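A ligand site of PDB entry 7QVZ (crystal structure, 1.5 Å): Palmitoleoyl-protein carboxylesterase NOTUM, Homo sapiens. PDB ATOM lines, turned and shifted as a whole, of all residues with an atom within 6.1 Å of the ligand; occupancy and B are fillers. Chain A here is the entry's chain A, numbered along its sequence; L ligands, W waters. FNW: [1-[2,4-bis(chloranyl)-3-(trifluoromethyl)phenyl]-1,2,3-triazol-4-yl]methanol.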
ATOM      1  N   GLY A  49     -10.101 -31.654  22.835  1.00  0.00           N
ATOM      2  CA  GLY A  49     -10.897 -30.622  22.206  1.00  0.00           C
ATOM      3  C   GLY A  49     -10.252 -29.245  22.256  1.00  0.00           C
ATOM      4  O   GLY A  49      -9.048 -29.096  22.516  1.00  0.00           O
ATOM      5  N   GLY A  50     -11.068 -28.229  21.990  1.00  0.00           N
ATOM      6  CA  GLY A  50     -10.573 -26.861  21.921  1.00  0.00           C
ATOM      7  C   GLY A  50     -10.945 -26.062  20.675  1.00  0.00           C
ATOM      8  O   GLY A  50     -10.063 -25.552  19.984  1.00  0.00           O
ATOM      9  N   TRP A  51     -12.238 -25.927  20.411  1.00  0.00           N
ATOM     10  CA  TRP A  51     -12.752 -25.084  19.312  1.00  0.00           C
ATOM     11  C   TRP A  51     -12.189 -25.572  17.968  1.00  0.00           C
ATOM     12  O   TRP A  51     -12.057 -26.788  17.766  1.00  0.00           O
ATOM     13  CB  TRP A  51     -12.589 -23.602  19.618  1.00  0.00           C
ATOM     14  CG  TRP A  51     -13.439 -23.168  20.759  1.00  0.00           C
ATOM     15  CD1 TRP A  51     -13.044 -22.991  22.056  1.00  0.00           C
ATOM     16  CD2 TRP A  51     -14.840 -22.883  20.724  1.00  0.00           C
ATOM     17  NE1 TRP A  51     -14.110 -22.604  22.823  1.00  0.00           N
ATOM     18  CE2 TRP A  51     -15.221 -22.526  22.037  1.00  0.00           C
ATOM     19  CE3 TRP A  51     -15.817 -22.883  19.713  1.00  0.00           C
ATOM     20  CZ2 TRP A  51     -16.536 -22.162  22.361  1.00  0.00           C
ATOM     21  CZ3 TRP A  51     -17.109 -22.523  20.039  1.00  0.00           C
ATOM     22  CH2 TRP A  51     -17.462 -22.182  21.353  1.00  0.00           C
ATOM     23  N   TYR A  52     -11.879 -24.658  17.054  1.00  0.00           N
ATOM     24  CA  TYR A  52     -11.581 -24.929  15.658  1.00  0.00           C
ATOM     25  C   TYR A  52     -11.286 -23.576  15.031  1.00  0.00           C
ATOM     26  O   TYR A  52     -11.463 -22.539  15.670  1.00  0.00           O
ATOM     27  CB  TYR A  52     -12.765 -25.607  14.939  1.00  0.00           C
ATOM     28  CG  TYR A  52     -14.119 -25.014  15.317  1.00  0.00           C
ATOM     29  CD1 TYR A  52     -14.955 -25.659  16.210  1.00  0.00           C
ATOM     30  CD2 TYR A  52     -14.536 -23.791  14.782  1.00  0.00           C
ATOM     31  CE1 TYR A  52     -16.188 -25.118  16.567  1.00  0.00           C
ATOM     32  CE2 TYR A  52     -15.767 -23.240  15.135  1.00  0.00           C
ATOM     33  CZ  TYR A  52     -16.578 -23.920  16.036  1.00  0.00           C
ATOM     34  OH  TYR A  52     -17.792 -23.401  16.401  1.00  0.00           O
ATOM     35  N   TYR A 105      -5.132 -32.508  20.041  1.00  0.00           N
ATOM     36  CA  TYR A 105      -5.904 -31.881  18.978  1.00  0.00           C
ATOM     37  C   TYR A 105      -5.044 -30.782  18.372  1.00  0.00           C
ATOM     38  O   TYR A 105      -4.810 -29.744  18.999  1.00  0.00           O
ATOM     39  CB  TYR A 105      -7.156 -31.295  19.592  1.00  0.00           C
ATOM     40  CG  TYR A 105      -8.135 -30.596  18.687  1.00  0.00           C
ATOM     41  CD1 TYR A 105      -8.471 -31.101  17.440  1.00  0.00           C
ATOM     42  CD2 TYR A 105      -8.791 -29.455  19.130  1.00  0.00           C
ATOM     43  CE1 TYR A 105      -9.425 -30.482  16.633  1.00  0.00           C
ATOM     44  CE2 TYR A 105      -9.732 -28.821  18.347  1.00  0.00           C
ATOM     45  CZ  TYR A 105     -10.057 -29.335  17.108  1.00  0.00           C
ATOM     46  OH  TYR A 105     -10.997 -28.677  16.364  1.00  0.00           O
ATOM     47  N   VAL A 110     -12.319 -30.098  14.213  1.00  0.00           N
ATOM     48  CA  VAL A 110     -13.279 -30.979  14.870  1.00  0.00           C
ATOM     49  C   VAL A 110     -13.005 -32.426  14.475  1.00  0.00           C
ATOM     50  O   VAL A 110     -13.919 -33.263  14.411  1.00  0.00           O
ATOM     51  CB  VAL A 110     -14.741 -30.557  14.594  1.00  0.00           C
ATOM     52  CG1 VAL A 110     -15.680 -31.168  15.628  1.00  0.00           C
ATOM     53  CG2 VAL A 110     -14.908 -29.020  14.613  1.00  0.00           C
ATOM     54  N   SER A 154     -13.517 -34.983  24.348  1.00  0.00           N
ATOM     55  CA  SER A 154     -14.237 -33.875  24.975  1.00  0.00           C
ATOM     56  C   SER A 154     -14.291 -32.666  24.059  1.00  0.00           C
ATOM     57  O   SER A 154     -13.331 -32.381  23.352  1.00  0.00           O
ATOM     58  CB  SER A 154     -13.547 -33.454  26.280  1.00  0.00           C
ATOM     59  OG  SER A 154     -13.605 -34.501  27.232  1.00  0.00           O
ATOM     60  N   SER A 155     -15.429 -31.970  24.098  1.00  0.00           N
ATOM     61  CA  SER A 155     -15.681 -30.749  23.329  1.00  0.00           C
ATOM     62  C   SER A 155     -15.506 -31.047  21.839  1.00  0.00           C
ATOM     63  O   SER A 155     -16.214 -31.939  21.342  1.00  0.00           O
ATOM     64  CB  SER A 155     -15.019 -29.486  23.917  1.00  0.00           C
ATOM     65  OG  SER A 155     -13.779 -29.156  23.317  1.00  0.00           O
ATOM     66  N   ALA A 156     -14.626 -30.358  21.107  1.00  0.00           N
ATOM     67  CA  ALA A 156     -14.430 -30.729  19.704  1.00  0.00           C
ATOM     68  C   ALA A 156     -14.065 -32.205  19.567  1.00  0.00           C
ATOM     69  O   ALA A 156     -14.406 -32.834  18.555  1.00  0.00           O
ATOM     70  CB  ALA A 156     -13.363 -29.843  19.030  1.00  0.00           C
ATOM     71  N   GLY A 157     -13.387 -32.769  20.569  1.00  0.00           N
ATOM     72  CA  GLY A 157     -13.076 -34.191  20.535  1.00  0.00           C
ATOM     73  C   GLY A 157     -14.296 -35.076  20.761  1.00  0.00           C
ATOM     74  O   GLY A 157     -14.327 -36.214  20.277  1.00  0.00           O
ATOM     75  N   THR A 159     -17.367 -34.289  19.592  1.00  0.00           N
ATOM     76  CA  THR A 159     -17.916 -34.358  18.240  1.00  0.00           C
ATOM     77  C   THR A 159     -17.047 -35.247  17.356  1.00  0.00           C
ATOM     78  O   THR A 159     -17.558 -36.006  16.533  1.00  0.00           O
ATOM     79  CB  THR A 159     -18.066 -32.945  17.659  1.00  0.00           C
ATOM     80  OG1 THR A 159     -18.719 -32.088  18.607  1.00  0.00           O
ATOM     81  CG2 THR A 159     -18.865 -32.980  16.358  1.00  0.00           C
ATOM     82  N   SER A 188     -19.419 -33.628  25.856  1.00  0.00           N
ATOM     83  CA  SER A 188     -19.524 -32.200  25.578  1.00  0.00           C
ATOM     84  C   SER A 188     -19.367 -31.895  24.090  1.00  0.00           C
ATOM     85  O   SER A 188     -18.845 -30.828  23.706  1.00  0.00           O
ATOM     86  CB  SER A 188     -18.511 -31.396  26.416  1.00  0.00           C
ATOM     87  OG  SER A 188     -18.723 -31.614  27.808  1.00  0.00           O
ATOM     88  N   GLY A 189     -19.825 -32.811  23.245  1.00  0.00           N
ATOM     89  CA  GLY A 189     -19.751 -32.654  21.808  1.00  0.00           C
ATOM     90  C   GLY A 189     -21.082 -32.781  21.116  1.00  0.00           C
ATOM     91  O   GLY A 189     -21.137 -32.976  19.901  1.00  0.00           O
ATOM     92  N   PHE A 191     -24.243 -30.853  20.205  1.00  0.00           N
ATOM     93  CA  PHE A 191     -24.691 -29.480  20.044  1.00  0.00           C
ATOM     94  C   PHE A 191     -25.997 -29.386  19.288  1.00  0.00           C
ATOM     95  O   PHE A 191     -26.390 -30.291  18.546  1.00  0.00           O
ATOM     96  CB  PHE A 191     -23.599 -28.645  19.359  1.00  0.00           C
ATOM     97  CG  PHE A 191     -22.362 -28.553  20.182  1.00  0.00           C
ATOM     98  CD1 PHE A 191     -22.324 -27.726  21.289  1.00  0.00           C
ATOM     99  CD2 PHE A 191     -21.268 -29.374  19.934  1.00  0.00           C
ATOM    100  CE1 PHE A 191     -21.186 -27.666  22.087  1.00  0.00           C
ATOM    101  CE2 PHE A 191     -20.140 -29.328  20.717  1.00  0.00           C
ATOM    102  CZ  PHE A 191     -20.101 -28.475  21.806  1.00  0.00           C
ATOM    103  N   LEU A 192     -26.698 -28.253  19.482  1.00  0.00           N
ATOM    104  CA  LEU A 192     -27.929 -27.953  18.778  1.00  0.00           C
ATOM    105  C   LEU A 192     -27.675 -26.864  17.747  1.00  0.00           C
ATOM    106  O   LEU A 192     -27.026 -25.853  18.052  1.00  0.00           O
ATOM    107  CB  LEU A 192     -28.997 -27.461  19.770  1.00  0.00           C
ATOM    108  CG  LEU A 192     -29.303 -28.452  20.903  1.00  0.00           C
ATOM    109  CD1 LEU A 192     -30.393 -27.888  21.809  1.00  0.00           C
ATOM    110  CD2 LEU A 192     -29.708 -29.804  20.328  1.00  0.00           C
ATOM    111  N   CYS A 208     -19.786 -17.274  16.457  1.00  0.00           N
ATOM    112  CA  CYS A 208     -20.442 -17.579  15.199  1.00  0.00           C
ATOM    113  C   CYS A 208     -21.549 -18.604  15.427  1.00  0.00           C
ATOM    114  O   CYS A 208     -21.367 -19.570  16.181  1.00  0.00           O
ATOM    115  CB  CYS A 208     -19.421 -18.140  14.200  1.00  0.00           C
ATOM    116  SG  CYS A 208     -20.095 -18.639  12.602  1.00  0.00           S
ATOM    117  N   ALA A 209     -22.703 -18.368  14.804  1.00  0.00           N
ATOM    118  CA  ALA A 209     -23.832 -19.280  14.937  1.00  0.00           C
ATOM    119  C   ALA A 209     -23.385 -20.702  14.592  1.00  0.00           C
ATOM    120  O   ALA A 209     -22.585 -20.885  13.663  1.00  0.00           O
ATOM    121  CB  ALA A 209     -24.960 -18.863  13.999  1.00  0.00           C
ATOM    122  N   PRO A 210     -23.873 -21.720  15.308  1.00  0.00           N
ATOM    123  CA  PRO A 210     -23.344 -23.073  15.089  1.00  0.00           C
ATOM    124  C   PRO A 210     -23.498 -23.588  13.657  1.00  0.00           C
ATOM    125  O   PRO A 210     -22.602 -24.279  13.165  1.00  0.00           O
ATOM    126  CB  PRO A 210     -24.102 -23.932  16.131  1.00  0.00           C
ATOM    127  CG  PRO A 210     -25.295 -23.107  16.526  1.00  0.00           C
ATOM    128  CD  PRO A 210     -24.887 -21.672  16.380  1.00  0.00           C
ATOM    129  N   THR A 211     -24.581 -23.236  12.973  1.00  0.00           N
ATOM    130  CA  THR A 211     -24.802 -23.735  11.614  1.00  0.00           C
ATOM    131  C   THR A 211     -23.781 -23.177  10.633  1.00  0.00           C
ATOM    132  O   THR A 211     -23.170 -23.925   9.859  1.00  0.00           O
ATOM    133  CB  THR A 211     -26.233 -23.405  11.177  1.00  0.00           C
ATOM    134  OG1 THR A 211     -27.165 -24.016  12.084  1.00  0.00           O
ATOM    135  CG2 THR A 211     -26.495 -23.951   9.780  1.00  0.00           C
ATOM    136  N   ALA A 213     -20.829 -21.731  11.193  1.00  0.00           N
ATOM    137  CA  ALA A 213     -19.472 -22.118  11.543  1.00  0.00           C
ATOM    138  C   ALA A 213     -19.097 -23.431  10.866  1.00  0.00           C
ATOM    139  O   ALA A 213     -18.034 -23.530  10.224  1.00  0.00           O
ATOM    140  CB  ALA A 213     -19.342 -22.265  13.063  1.00  0.00           C
ATOM    141  N   ILE A 214     -19.957 -24.440  10.965  1.00  0.00           N
ATOM    142  CA  ILE A 214     -19.611 -25.758  10.449  1.00  0.00           C
ATOM    143  C   ILE A 214     -19.659 -25.777   8.930  1.00  0.00           C
ATOM    144  O   ILE A 214     -18.833 -26.420   8.279  1.00  0.00           O
ATOM    145  CB  ILE A 214     -20.511 -26.825  11.099  1.00  0.00           C
ATOM    146  CG1 ILE A 214     -20.326 -26.810  12.623  1.00  0.00           C
ATOM    147  CG2 ILE A 214     -20.206 -28.207  10.528  1.00  0.00           C
ATOM    148  CD1 ILE A 214     -18.902 -26.915  13.056  1.00  0.00           C
ATOM    149  N   PHE A 242     -22.310 -32.958  11.788  1.00  0.00           N
ATOM    150  CA  PHE A 242     -21.580 -32.518  12.979  1.00  0.00           C
ATOM    151  C   PHE A 242     -22.487 -32.340  14.184  1.00  0.00           C
ATOM    152  O   PHE A 242     -21.982 -32.117  15.295  1.00  0.00           O
ATOM    153  CB  PHE A 242     -20.881 -31.180  12.709  1.00  0.00           C
ATOM    154  CG  PHE A 242     -19.618 -31.298  11.933  1.00  0.00           C
ATOM    155  CD1 PHE A 242     -19.620 -31.770  10.624  1.00  0.00           C
ATOM    156  CD2 PHE A 242     -18.414 -30.847  12.461  1.00  0.00           C
ATOM    157  CE1 PHE A 242     -18.440 -31.864   9.903  1.00  0.00           C
ATOM    158  CE2 PHE A 242     -17.234 -30.924  11.725  1.00  0.00           C
ATOM    159  CZ  PHE A 242     -17.254 -31.424  10.453  1.00  0.00           C
ATOM    160  N   PHE A 243     -23.800 -32.473  14.005  1.00  0.00           N
ATOM    161  CA  PHE A 243     -24.763 -32.282  15.086  1.00  0.00           C
ATOM    162  C   PHE A 243     -25.223 -33.637  15.610  1.00  0.00           C
ATOM    163  O   PHE A 243     -25.848 -34.408  14.877  1.00  0.00           O
ATOM    164  CB  PHE A 243     -25.897 -31.386  14.625  1.00  0.00           C
ATOM    165  CG  PHE A 243     -25.423 -29.986  14.444  1.00  0.00           C
ATOM    166  CD1 PHE A 243     -25.393 -29.114  15.522  1.00  0.00           C
ATOM    167  CD2 PHE A 243     -24.846 -29.603  13.249  1.00  0.00           C
ATOM    168  CE1 PHE A 243     -24.875 -27.836  15.384  1.00  0.00           C
ATOM    169  CE2 PHE A 243     -24.316 -28.343  13.099  1.00  0.00           C
ATOM    170  CZ  PHE A 243     -24.337 -27.451  14.173  1.00  0.00           C
ATOM    171  N   ASP A 263     -24.548 -26.395  28.253  1.00  0.00           N
ATOM    172  CA  ASP A 263     -23.125 -26.395  27.962  1.00  0.00           C
ATOM    173  C   ASP A 263     -22.632 -24.986  27.624  1.00  0.00           C
ATOM    174  O   ASP A 263     -23.268 -24.274  26.838  1.00  0.00           O
ATOM    175  CB  ASP A 263     -22.860 -27.347  26.788  1.00  0.00           C
ATOM    176  CG  ASP A 263     -21.399 -27.462  26.461  1.00  0.00           C
ATOM    177  OD1 ASP A 263     -20.889 -26.665  25.639  1.00  0.00           O
ATOM    178  OD2 ASP A 263     -20.746 -28.346  27.031  1.00  0.00           O
ATOM    179  N   ALA A 265     -20.123 -23.883  25.865  1.00  0.00           N
ATOM    180  CA  ALA A 265     -19.818 -23.635  24.456  1.00  0.00           C
ATOM    181  C   ALA A 265     -21.089 -23.476  23.623  1.00  0.00           C
ATOM    182  O   ALA A 265     -21.130 -22.667  22.672  1.00  0.00           O
ATOM    183  CB  ALA A 265     -18.942 -24.752  23.894  1.00  0.00           C
ATOM    184  N   GLN A 266     -22.133 -24.255  23.922  1.00  0.00           N
ATOM    185  CA  GLN A 266     -23.436 -24.047  23.285  1.00  0.00           C
ATOM    186  C   GLN A 266     -23.942 -22.624  23.534  1.00  0.00           C
ATOM    187  O   GLN A 266     -24.344 -21.918  22.607  1.00  0.00           O
ATOM    188  CB  GLN A 266     -24.445 -25.067  23.816  1.00  0.00           C
ATOM    189  CG  GLN A 266     -25.845 -24.917  23.238  1.00  0.00           C
ATOM    190  CD  GLN A 266     -25.976 -25.486  21.820  1.00  0.00           C
ATOM    191  OE1 GLN A 266     -25.630 -26.642  21.571  1.00  0.00           O
ATOM    192  NE2 GLN A 266     -26.464 -24.666  20.894  1.00  0.00           N
ATOM    193  N   VAL A 269     -21.853 -20.012  21.456  1.00  0.00           N
ATOM    194  CA  VAL A 269     -22.243 -19.880  20.060  1.00  0.00           C
ATOM    195  C   VAL A 269     -23.663 -19.357  19.922  1.00  0.00           C
ATOM    196  O   VAL A 269     -24.013 -18.806  18.882  1.00  0.00           O
ATOM    197  CB  VAL A 269     -22.017 -21.160  19.231  1.00  0.00           C
ATOM    198  CG1 VAL A 269     -20.543 -21.559  19.258  1.00  0.00           C
ATOM    199  CG2 VAL A 269     -22.902 -22.303  19.722  1.00  0.00           C
HETATM  200  C01 FNW L   1     -18.065 -27.469  18.913  1.00  0.00           C
HETATM  201  C05 FNW L   1     -15.847 -26.519  21.569  1.00  0.00           C
HETATM  202  C06 FNW L   1     -15.391 -25.998  22.938  1.00  0.00           C
HETATM  203  C08 FNW L   1     -17.135 -26.643  21.072  1.00  0.00           C
HETATM  204  C09 FNW L   1     -17.949 -28.663  18.250  1.00  0.00           C
HETATM  205  C10 FNW L   1     -18.892 -29.032  17.344  1.00  0.00           C
HETATM  206  C11 FNW L   1     -19.972 -28.218  17.091  1.00  0.00           C
HETATM  207  C13 FNW L   1     -20.107 -27.002  17.746  1.00  0.00           C
HETATM  208  C14 FNW L   1     -21.289 -26.068  17.502  1.00  0.00           C
HETATM  209  C18 FNW L   1     -19.149 -26.650  18.672  1.00  0.00           C
HETATM  210  F15 FNW L   1     -22.029 -26.494  16.447  1.00  0.00           F
HETATM  211  F16 FNW L   1     -20.863 -24.790  17.215  1.00  0.00           F
HETATM  212  F17 FNW L   1     -22.108 -25.973  18.573  1.00  0.00           F
HETATM  213  N02 FNW L   1     -17.040 -27.136  19.857  1.00  0.00           N
HETATM  214  N03 FNW L   1     -15.731 -27.332  19.552  1.00  0.00           N
HETATM  215  N04 FNW L   1     -15.020 -26.957  20.633  1.00  0.00           N
HETATM  216  O07 FNW L   1     -14.091 -26.495  23.148  1.00  0.00           O
HETATM  217 CL12 FNW L   1     -21.165 -28.779  15.907  1.00  0.00          CL
HETATM  218 CL19 FNW L   1     -19.292 -25.127  19.541  1.00  0.00          CL
HETATM  219  O   HOH W   1     -12.671 -25.354  25.094  1.00  0.00           O
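A fluorine (F16) of the ligand lies close to the side-chain hydroxyl (OH) of Tyr 52 (3.5 Å). Merely in contact with the ligand: Phe 191, Pro 210, Thr 159, Phe 243, Phe 242, Gly 50, Val 269, Ala 265 and Ile 214. Hydrophobic or aromatic side chains within 4 Å of the ligand: Trp 51, Tyr 52, Ala 156, Phe 191, Pro 210, Ile 214, Phe 243, Ala 265 and Val 269. Within 4 Å of the ligand: Gly 50, Trp 51, Tyr 52, Ser 155, Ala 156, Thr 159, Phe 191, Pro 210, Ile 214, Phe 242, Phe 243, Ala 265 and Val 269. Along chain A the residues within 4 Å of the ligand span positions 50 to 269.
The side-chain carboxylate of Asp 263 is in hydrogen-bond range of the backbone NH of Ala 265, 2.9 Å away. The backbone carbonyl oxygen of Trp 51 is in hydrogen-bond range of the side-chain hydroxyl of Tyr 105. The side-chain hydroxyl (OG) of Ser 155 sits at hydrogen-bond distance from the backbone NH (N) of Gly 50 (3.2 Å). The backbone carbonyl oxygen (O) of Gly 189 is in hydrogen-bond range of the side-chain hydroxyl (OG1) of Thr 159.
N04 of the ligand sits at hydrogen-bond distance from N of Trp 51 (3.0 Å). The backbone NH (N) of Ala 156 lies within hydrogen-bond range of a nitrogen (N04) of the ligand. OG of Ser 155 lies within hydrogen-bond range of O07 of the ligand (2.7 Å).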
